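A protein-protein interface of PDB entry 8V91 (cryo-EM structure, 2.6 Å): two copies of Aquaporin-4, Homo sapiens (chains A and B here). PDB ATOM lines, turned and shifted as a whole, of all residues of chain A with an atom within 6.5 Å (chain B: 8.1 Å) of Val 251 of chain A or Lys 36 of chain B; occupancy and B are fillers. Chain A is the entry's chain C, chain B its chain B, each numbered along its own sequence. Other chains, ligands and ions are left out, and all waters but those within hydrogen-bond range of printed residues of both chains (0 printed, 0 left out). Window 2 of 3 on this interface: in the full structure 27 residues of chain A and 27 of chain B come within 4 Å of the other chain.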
ATOM      1  N   GLY A 246      22.565  33.741  14.177  1.00  0.00           N
ATOM      2  CA  GLY A 246      21.677  34.404  15.119  1.00  0.00           C
ATOM      3  C   GLY A 246      20.304  33.762  15.188  1.00  0.00           C
ATOM      4  O   GLY A 246      19.725  33.632  16.268  1.00  0.00           O
ATOM      5  N   LEU A 247      19.762  33.362  14.036  1.00  0.00           N
ATOM      6  CA  LEU A 247      18.444  32.737  14.017  1.00  0.00           C
ATOM      7  C   LEU A 247      18.443  31.420  14.781  1.00  0.00           C
ATOM      8  O   LEU A 247      17.519  31.142  15.554  1.00  0.00           O
ATOM      9  CB  LEU A 247      17.990  32.518  12.574  1.00  0.00           C
ATOM     10  CG  LEU A 247      16.562  32.928  12.219  1.00  0.00           C
ATOM     11  CD1 LEU A 247      16.263  34.330  12.719  1.00  0.00           C
ATOM     12  CD2 LEU A 247      16.347  32.841  10.720  1.00  0.00           C
ATOM     13  N   TYR A 248      19.471  30.596  14.581  1.00  0.00           N
ATOM     14  CA  TYR A 248      19.526  29.303  15.253  1.00  0.00           C
ATOM     15  C   TYR A 248      19.748  29.466  16.752  1.00  0.00           C
ATOM     16  O   TYR A 248      19.040  28.864  17.565  1.00  0.00           O
ATOM     17  CB  TYR A 248      20.629  28.443  14.636  1.00  0.00           C
ATOM     18  CG  TYR A 248      20.627  27.007  15.105  1.00  0.00           C
ATOM     19  CD1 TYR A 248      19.893  26.041  14.437  1.00  0.00           C
ATOM     20  CD2 TYR A 248      21.356  26.621  16.220  1.00  0.00           C
ATOM     21  CE1 TYR A 248      19.888  24.729  14.862  1.00  0.00           C
ATOM     22  CE2 TYR A 248      21.355  25.313  16.655  1.00  0.00           C
ATOM     23  CZ  TYR A 248      20.620  24.370  15.972  1.00  0.00           C
ATOM     24  OH  TYR A 248      20.619  23.065  16.403  1.00  0.00           O
ATOM     25  N   GLU A 249      20.726  30.288  17.136  1.00  0.00           N
ATOM     26  CA  GLU A 249      21.137  30.361  18.533  1.00  0.00           C
ATOM     27  C   GLU A 249      20.164  31.156  19.396  1.00  0.00           C
ATOM     28  O   GLU A 249      20.003  30.840  20.580  1.00  0.00           O
ATOM     29  CB  GLU A 249      22.534  30.973  18.636  1.00  0.00           C
ATOM     30  CG  GLU A 249      23.649  30.051  18.184  1.00  0.00           C
ATOM     31  CD  GLU A 249      23.815  28.848  19.091  1.00  0.00           C
ATOM     32  OE1 GLU A 249      23.972  29.043  20.314  1.00  0.00           O
ATOM     33  OE2 GLU A 249      23.790  27.707  18.582  1.00  0.00           O
ATOM     34  N   TYR A 250      19.517  32.180  18.842  1.00  0.00           N
ATOM     35  CA  TYR A 250      18.733  33.104  19.648  1.00  0.00           C
ATOM     36  C   TYR A 250      17.237  33.064  19.375  1.00  0.00           C
ATOM     37  O   TYR A 250      16.483  33.742  20.081  1.00  0.00           O
ATOM     38  CB  TYR A 250      19.241  34.538  19.447  1.00  0.00           C
ATOM     39  CG  TYR A 250      20.699  34.718  19.804  1.00  0.00           C
ATOM     40  CD1 TYR A 250      21.163  34.412  21.074  1.00  0.00           C
ATOM     41  CD2 TYR A 250      21.610  35.194  18.872  1.00  0.00           C
ATOM     42  CE1 TYR A 250      22.492  34.574  21.407  1.00  0.00           C
ATOM     43  CE2 TYR A 250      22.940  35.359  19.195  1.00  0.00           C
ATOM     44  CZ  TYR A 250      23.376  35.047  20.465  1.00  0.00           C
ATOM     45  OH  TYR A 250      24.701  35.210  20.795  1.00  0.00           O
ATOM     46  N   VAL A 251      16.781  32.298  18.385  1.00  0.00           N
ATOM     47  CA  VAL A 251      15.357  32.240  18.077  1.00  0.00           C
ATOM     48  C   VAL A 251      14.865  30.801  18.133  1.00  0.00           C
ATOM     49  O   VAL A 251      13.924  30.482  18.867  1.00  0.00           O
ATOM     50  CB  VAL A 251      15.056  32.865  16.702  1.00  0.00           C
ATOM     51  CG1 VAL A 251      13.575  32.758  16.389  1.00  0.00           C
ATOM     52  CG2 VAL A 251      15.510  34.314  16.664  1.00  0.00           C
ATOM     53  N   PHE A 252      15.499  29.919  17.358  1.00  0.00           N
ATOM     54  CA  PHE A 252      15.002  28.554  17.226  1.00  0.00           C
ATOM     55  C   PHE A 252      15.371  27.699  18.431  1.00  0.00           C
ATOM     56  O   PHE A 252      14.509  27.037  19.018  1.00  0.00           O
ATOM     57  CB  PHE A 252      15.533  27.928  15.937  1.00  0.00           C
ATOM     58  CG  PHE A 252      14.764  28.325  14.712  1.00  0.00           C
ATOM     59  CD1 PHE A 252      13.432  27.979  14.571  1.00  0.00           C
ATOM     60  CD2 PHE A 252      15.370  29.047  13.701  1.00  0.00           C
ATOM     61  CE1 PHE A 252      12.722  28.344  13.447  1.00  0.00           C
ATOM     62  CE2 PHE A 252      14.666  29.414  12.573  1.00  0.00           C
ATOM     63  CZ  PHE A 252      13.340  29.062  12.447  1.00  0.00           C
ATOM     64  N   CYS A 253      16.645  27.701  18.818  1.00  0.00           N
ATOM     65  CA  CYS A 253      17.135  26.897  19.937  1.00  0.00           C
ATOM     66  C   CYS A 253      17.917  27.794  20.887  1.00  0.00           C
ATOM     67  O   CYS A 253      19.155  27.777  20.899  1.00  0.00           O
ATOM     68  CB  CYS A 253      17.995  25.732  19.444  1.00  0.00           C
ATOM     69  SG  CYS A 253      17.177  24.658  18.244  1.00  0.00           S
ATOM     70  N   PRO A 254      17.221  28.597  21.706  1.00  0.00           N
ATOM     71  CA  PRO A 254      17.882  29.496  22.656  1.00  0.00           C
ATOM     72  C   PRO A 254      18.345  28.778  23.921  1.00  0.00           C
ATOM     73  O   PRO A 254      19.063  27.784  23.818  1.00  0.00           O
ATOM     74  CB  PRO A 254      16.791  30.515  22.978  1.00  0.00           C
ATOM     75  CG  PRO A 254      15.531  29.737  22.857  1.00  0.00           C
ATOM     76  CD  PRO A 254      15.754  28.731  21.755  1.00  0.00           C
ATOM     77  N   GLN B  32       6.369  30.302  21.843  1.00  0.00           N
ATOM     78  CA  GLN B  32       5.594  29.079  21.666  1.00  0.00           C
ATOM     79  C   GLN B  32       6.234  28.181  20.616  1.00  0.00           C
ATOM     80  O   GLN B  32       6.611  28.642  19.540  1.00  0.00           O
ATOM     81  CB  GLN B  32       4.153  29.408  21.273  1.00  0.00           C
ATOM     82  CG  GLN B  32       3.233  28.200  21.213  1.00  0.00           C
ATOM     83  CD  GLN B  32       1.785  28.582  20.984  1.00  0.00           C
ATOM     84  OE1 GLN B  32       1.440  29.763  20.951  1.00  0.00           O
ATOM     85  NE2 GLN B  32       0.926  27.582  20.825  1.00  0.00           N
ATOM     86  N   ALA B  33       6.360  26.891  20.937  1.00  0.00           N
ATOM     87  CA  ALA B  33       6.943  25.944  19.994  1.00  0.00           C
ATOM     88  C   ALA B  33       6.069  25.734  18.767  1.00  0.00           C
ATOM     89  O   ALA B  33       6.583  25.329  17.719  1.00  0.00           O
ATOM     90  CB  ALA B  33       7.203  24.605  20.684  1.00  0.00           C
ATOM     91  N   PHE B  34       4.762  25.990  18.872  1.00  0.00           N
ATOM     92  CA  PHE B  34       3.885  25.864  17.712  1.00  0.00           C
ATOM     93  C   PHE B  34       4.251  26.879  16.635  1.00  0.00           C
ATOM     94  O   PHE B  34       4.350  26.537  15.452  1.00  0.00           O
ATOM     95  CB  PHE B  34       2.427  26.033  18.143  1.00  0.00           C
ATOM     96  CG  PHE B  34       1.430  25.722  17.061  1.00  0.00           C
ATOM     97  CD1 PHE B  34       1.756  24.878  16.013  1.00  0.00           C
ATOM     98  CD2 PHE B  34       0.165  26.278  17.094  1.00  0.00           C
ATOM     99  CE1 PHE B  34       0.840  24.600  15.021  1.00  0.00           C
ATOM    100  CE2 PHE B  34      -0.756  26.000  16.105  1.00  0.00           C
ATOM    101  CZ  PHE B  34      -0.418  25.159  15.068  1.00  0.00           C
ATOM    102  N   TRP B  35       4.457  28.137  17.030  1.00  0.00           N
ATOM    103  CA  TRP B  35       4.820  29.160  16.055  1.00  0.00           C
ATOM    104  C   TRP B  35       6.201  28.897  15.469  1.00  0.00           C
ATOM    105  O   TRP B  35       6.443  29.170  14.289  1.00  0.00           O
ATOM    106  CB  TRP B  35       4.758  30.545  16.698  1.00  0.00           C
ATOM    107  CG  TRP B  35       5.814  31.483  16.203  1.00  0.00           C
ATOM    108  CD1 TRP B  35       5.768  32.246  15.074  1.00  0.00           C
ATOM    109  CD2 TRP B  35       7.071  31.769  16.829  1.00  0.00           C
ATOM    110  NE1 TRP B  35       6.920  32.983  14.952  1.00  0.00           N
ATOM    111  CE2 TRP B  35       7.737  32.709  16.017  1.00  0.00           C
ATOM    112  CE3 TRP B  35       7.699  31.319  17.994  1.00  0.00           C
ATOM    113  CZ2 TRP B  35       8.998  33.206  16.334  1.00  0.00           C
ATOM    114  CZ3 TRP B  35       8.950  31.815  18.307  1.00  0.00           C
ATOM    115  CH2 TRP B  35       9.586  32.748  17.480  1.00  0.00           C
ATOM    116  N   LYS B  36       7.121  28.371  16.280  1.00  0.00           N
ATOM    117  CA  LYS B  36       8.452  28.053  15.775  1.00  0.00           C
ATOM    118  C   LYS B  36       8.409  26.884  14.798  1.00  0.00           C
ATOM    119  O   LYS B  36       9.150  26.869  13.808  1.00  0.00           O
ATOM    120  CB  LYS B  36       9.395  27.750  16.939  1.00  0.00           C
ATOM    121  CG  LYS B  36      10.509  28.770  17.109  1.00  0.00           C
ATOM    122  CD  LYS B  36      10.934  28.902  18.562  1.00  0.00           C
ATOM    123  CE  LYS B  36      11.123  27.547  19.217  1.00  0.00           C
ATOM    124  NZ  LYS B  36      11.472  27.679  20.659  1.00  0.00           N
ATOM    125  N   ALA B  37       7.557  25.890  15.063  1.00  0.00           N
ATOM    126  CA  ALA B  37       7.449  24.750  14.160  1.00  0.00           C
ATOM    127  C   ALA B  37       6.896  25.166  12.802  1.00  0.00           C
ATOM    128  O   ALA B  37       7.394  24.722  11.761  1.00  0.00           O
ATOM    129  CB  ALA B  37       6.574  23.665  14.786  1.00  0.00           C
ATOM    130  N   VAL B  38       5.863  26.011  12.792  1.00  0.00           N
ATOM    131  CA  VAL B  38       5.292  26.471  11.530  1.00  0.00           C
ATOM    132  C   VAL B  38       6.286  27.350  10.782  1.00  0.00           C
ATOM    133  O   VAL B  38       6.429  27.245   9.558  1.00  0.00           O
ATOM    134  CB  VAL B  38       3.962  27.203  11.782  1.00  0.00           C
ATOM    135  CG1 VAL B  38       3.434  27.800  10.493  1.00  0.00           C
ATOM    136  CG2 VAL B  38       2.944  26.253  12.384  1.00  0.00           C
ATOM    137  N   THR B  39       6.988  28.227  11.504  1.00  0.00           N
ATOM    138  CA  THR B  39       7.987  29.081  10.869  1.00  0.00           C
ATOM    139  C   THR B  39       9.121  28.256  10.277  1.00  0.00           C
ATOM    140  O   THR B  39       9.619  28.565   9.188  1.00  0.00           O
ATOM    141  CB  THR B  39       8.530  30.091  11.877  1.00  0.00           C
ATOM    142  OG1 THR B  39       7.454  30.896  12.371  1.00  0.00           O
ATOM    143  CG2 THR B  39       9.564  30.990  11.225  1.00  0.00           C
ATOM    144  N   ALA B  40       9.542  27.203  10.979  1.00  0.00           N
ATOM    145  CA  ALA B  40      10.587  26.334  10.448  1.00  0.00           C
ATOM    146  C   ALA B  40      10.138  25.655   9.162  1.00  0.00           C
ATOM    147  O   ALA B  40      10.920  25.531   8.213  1.00  0.00           O
ATOM    148  CB  ALA B  40      10.989  25.294  11.492  1.00  0.00           C
ATOM    149  N   GLU B  41       8.881  25.205   9.112  1.00  0.00           N
ATOM    150  CA  GLU B  41       8.369  24.574   7.899  1.00  0.00           C
ATOM    151  C   GLU B  41       8.312  25.561   6.741  1.00  0.00           C
ATOM    152  O   GLU B  41       8.643  25.210   5.603  1.00  0.00           O
ATOM    153  CB  GLU B  41       6.990  23.972   8.159  1.00  0.00           C
ATOM    154  CG  GLU B  41       7.029  22.706   8.986  1.00  0.00           C
ATOM    155  CD  GLU B  41       7.413  21.484   8.171  1.00  0.00           C
ATOM    156  OE1 GLU B  41       7.087  21.441   6.967  1.00  0.00           O
ATOM    157  OE2 GLU B  41       8.042  20.564   8.736  1.00  0.00           O
ATOM    158  N   PHE B  42       7.885  26.797   7.006  1.00  0.00           N
ATOM    159  CA  PHE B  42       7.884  27.813   5.959  1.00  0.00           C
ATOM    160  C   PHE B  42       9.295  28.099   5.464  1.00  0.00           C
ATOM    161  O   PHE B  42       9.528  28.209   4.255  1.00  0.00           O
ATOM    162  CB  PHE B  42       7.222  29.093   6.468  1.00  0.00           C
ATOM    163  CG  PHE B  42       7.510  30.302   5.622  1.00  0.00           C
ATOM    164  CD1 PHE B  42       6.758  30.567   4.492  1.00  0.00           C
ATOM    165  CD2 PHE B  42       8.523  31.181   5.965  1.00  0.00           C
ATOM    166  CE1 PHE B  42       7.020  31.677   3.713  1.00  0.00           C
ATOM    167  CE2 PHE B  42       8.789  32.291   5.190  1.00  0.00           C
ATOM    168  CZ  PHE B  42       8.036  32.539   4.063  1.00  0.00           C
ATOM    169  N   LEU B  43      10.251  28.223   6.385  1.00  0.00           N
ATOM    170  CA  LEU B  43      11.615  28.552   5.989  1.00  0.00           C
ATOM    171  C   LEU B  43      12.299  27.368   5.315  1.00  0.00           C
ATOM    172  O   LEU B  43      12.982  27.539   4.298  1.00  0.00           O
ATOM    173  CB  LEU B  43      12.410  29.020   7.206  1.00  0.00           C
ATOM    174  CG  LEU B  43      13.856  29.455   6.972  1.00  0.00           C
ATOM    175  CD1 LEU B  43      13.903  30.638   6.024  1.00  0.00           C
ATOM    176  CD2 LEU B  43      14.521  29.800   8.292  1.00  0.00           C
ATOM    177  N   PHE B  88      16.245  21.182  10.112  1.00  0.00           N
ATOM    178  CA  PHE B  88      14.982  21.474  10.781  1.00  0.00           C
ATOM    179  C   PHE B  88      14.256  20.220  11.252  1.00  0.00           C
ATOM    180  O   PHE B  88      13.055  20.277  11.534  1.00  0.00           O
ATOM    181  CB  PHE B  88      14.073  22.283   9.854  1.00  0.00           C
ATOM    182  CG  PHE B  88      14.581  23.665   9.560  1.00  0.00           C
ATOM    183  CD1 PHE B  88      14.488  24.668  10.508  1.00  0.00           C
ATOM    184  CD2 PHE B  88      15.158  23.959   8.338  1.00  0.00           C
ATOM    185  CE1 PHE B  88      14.950  25.937  10.239  1.00  0.00           C
ATOM    186  CE2 PHE B  88      15.622  25.229   8.062  1.00  0.00           C
ATOM    187  CZ  PHE B  88      15.521  26.218   9.014  1.00  0.00           C
ATOM    188  N   ILE B  91      13.053  20.610  14.977  1.00  0.00           N
ATOM    189  CA  ILE B  91      12.242  21.784  15.280  1.00  0.00           C
ATOM    190  C   ILE B  91      10.776  21.562  14.930  1.00  0.00           C
ATOM    191  O   ILE B  91       9.891  21.820  15.744  1.00  0.00           O
ATOM    192  CB  ILE B  91      12.807  23.027  14.560  1.00  0.00           C
ATOM    193  CG1 ILE B  91      14.260  23.265  14.974  1.00  0.00           C
ATOM    194  CG2 ILE B  91      11.961  24.248  14.874  1.00  0.00           C
ATOM    195  CD1 ILE B  91      14.961  24.331  14.167  1.00  0.00           C
ATOM    196  N   SER B  92      10.500  21.078  13.719  1.00  0.00           N
ATOM    197  CA  SER B  92       9.129  20.886  13.269  1.00  0.00           C
ATOM    198  C   SER B  92       8.828  19.471  12.801  1.00  0.00           C
ATOM    199  O   SER B  92       7.687  19.198  12.413  1.00  0.00           O
ATOM    200  CB  SER B  92       8.798  21.861  12.131  1.00  0.00           C
ATOM    201  OG  SER B  92       9.515  21.526  10.955  1.00  0.00           O
ATOM    202  N   TYR B 118       0.766  23.606   8.868  1.00  0.00           N
ATOM    203  CA  TYR B 118       1.893  23.053   8.123  1.00  0.00           C
ATOM    204  C   TYR B 118       1.684  23.185   6.622  1.00  0.00           C
ATOM    205  O   TYR B 118       2.576  23.640   5.896  1.00  0.00           O
ATOM    206  CB  TYR B 118       2.102  21.588   8.506  1.00  0.00           C
ATOM    207  CG  TYR B 118       3.030  21.359   9.676  1.00  0.00           C
ATOM    208  CD1 TYR B 118       2.711  21.811  10.946  1.00  0.00           C
ATOM    209  CD2 TYR B 118       4.209  20.645   9.515  1.00  0.00           C
ATOM    210  CE1 TYR B 118       3.557  21.591  12.012  1.00  0.00           C
ATOM    211  CE2 TYR B 118       5.055  20.414  10.577  1.00  0.00           C
ATOM    212  CZ  TYR B 118       4.725  20.889  11.823  1.00  0.00           C
ATOM    213  OH  TYR B 118       5.570  20.661  12.882  1.00  0.00           O
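The backbone NH (N) of Phe 252 of chain A sits at hydrogen-bond distance from the backbone carbonyl oxygen (O) of Leu 247 of chain A (3.0 Å).
O of Val 251 of chain A touches CD of Lys 36 of chain B (3.4 Å). Phe 252 of chain A touches Lys 36 of chain B. Ile 91 of chain B touches Phe 252 of chain A (CD1 to CD1, 3.98 Å).
Of the printed residues of chain B, Phe 252 of chain A touches Lys 36 (3.4 Å) and Ile 91 (3.98 Å). Lys 36 of chain B touches just these residues of chain A: Val 251 (3.4 Å) and Phe 252 (3.4 Å). Leu 43 of chain B touches none of the printed residues of chain A. Of the printed residues of chain A, Ile 91 of chain B touches Phe 252 (3.98 Å). The nearest printed residue of chain B that does not touch Phe 252 of chain A is Ala 40 of chain B (4.02 Å).
Printed residues of chain B that touch a printed residue of chain A: Lys 36 and Ile 91. Hydrophobic or aromatic side chains of chain B within 4 Å of the printed part of chain A: Ile 91. Hydrophobic or aromatic side chains of chain A that line the printed part of chain B: Phe 252. Among the printed residues, 3 pairs touch across the chains.
No position is printed for both chains. Of the 3 pairs that touch across the chains among the printed residues, none has its exchanged pair printed and touching as well.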
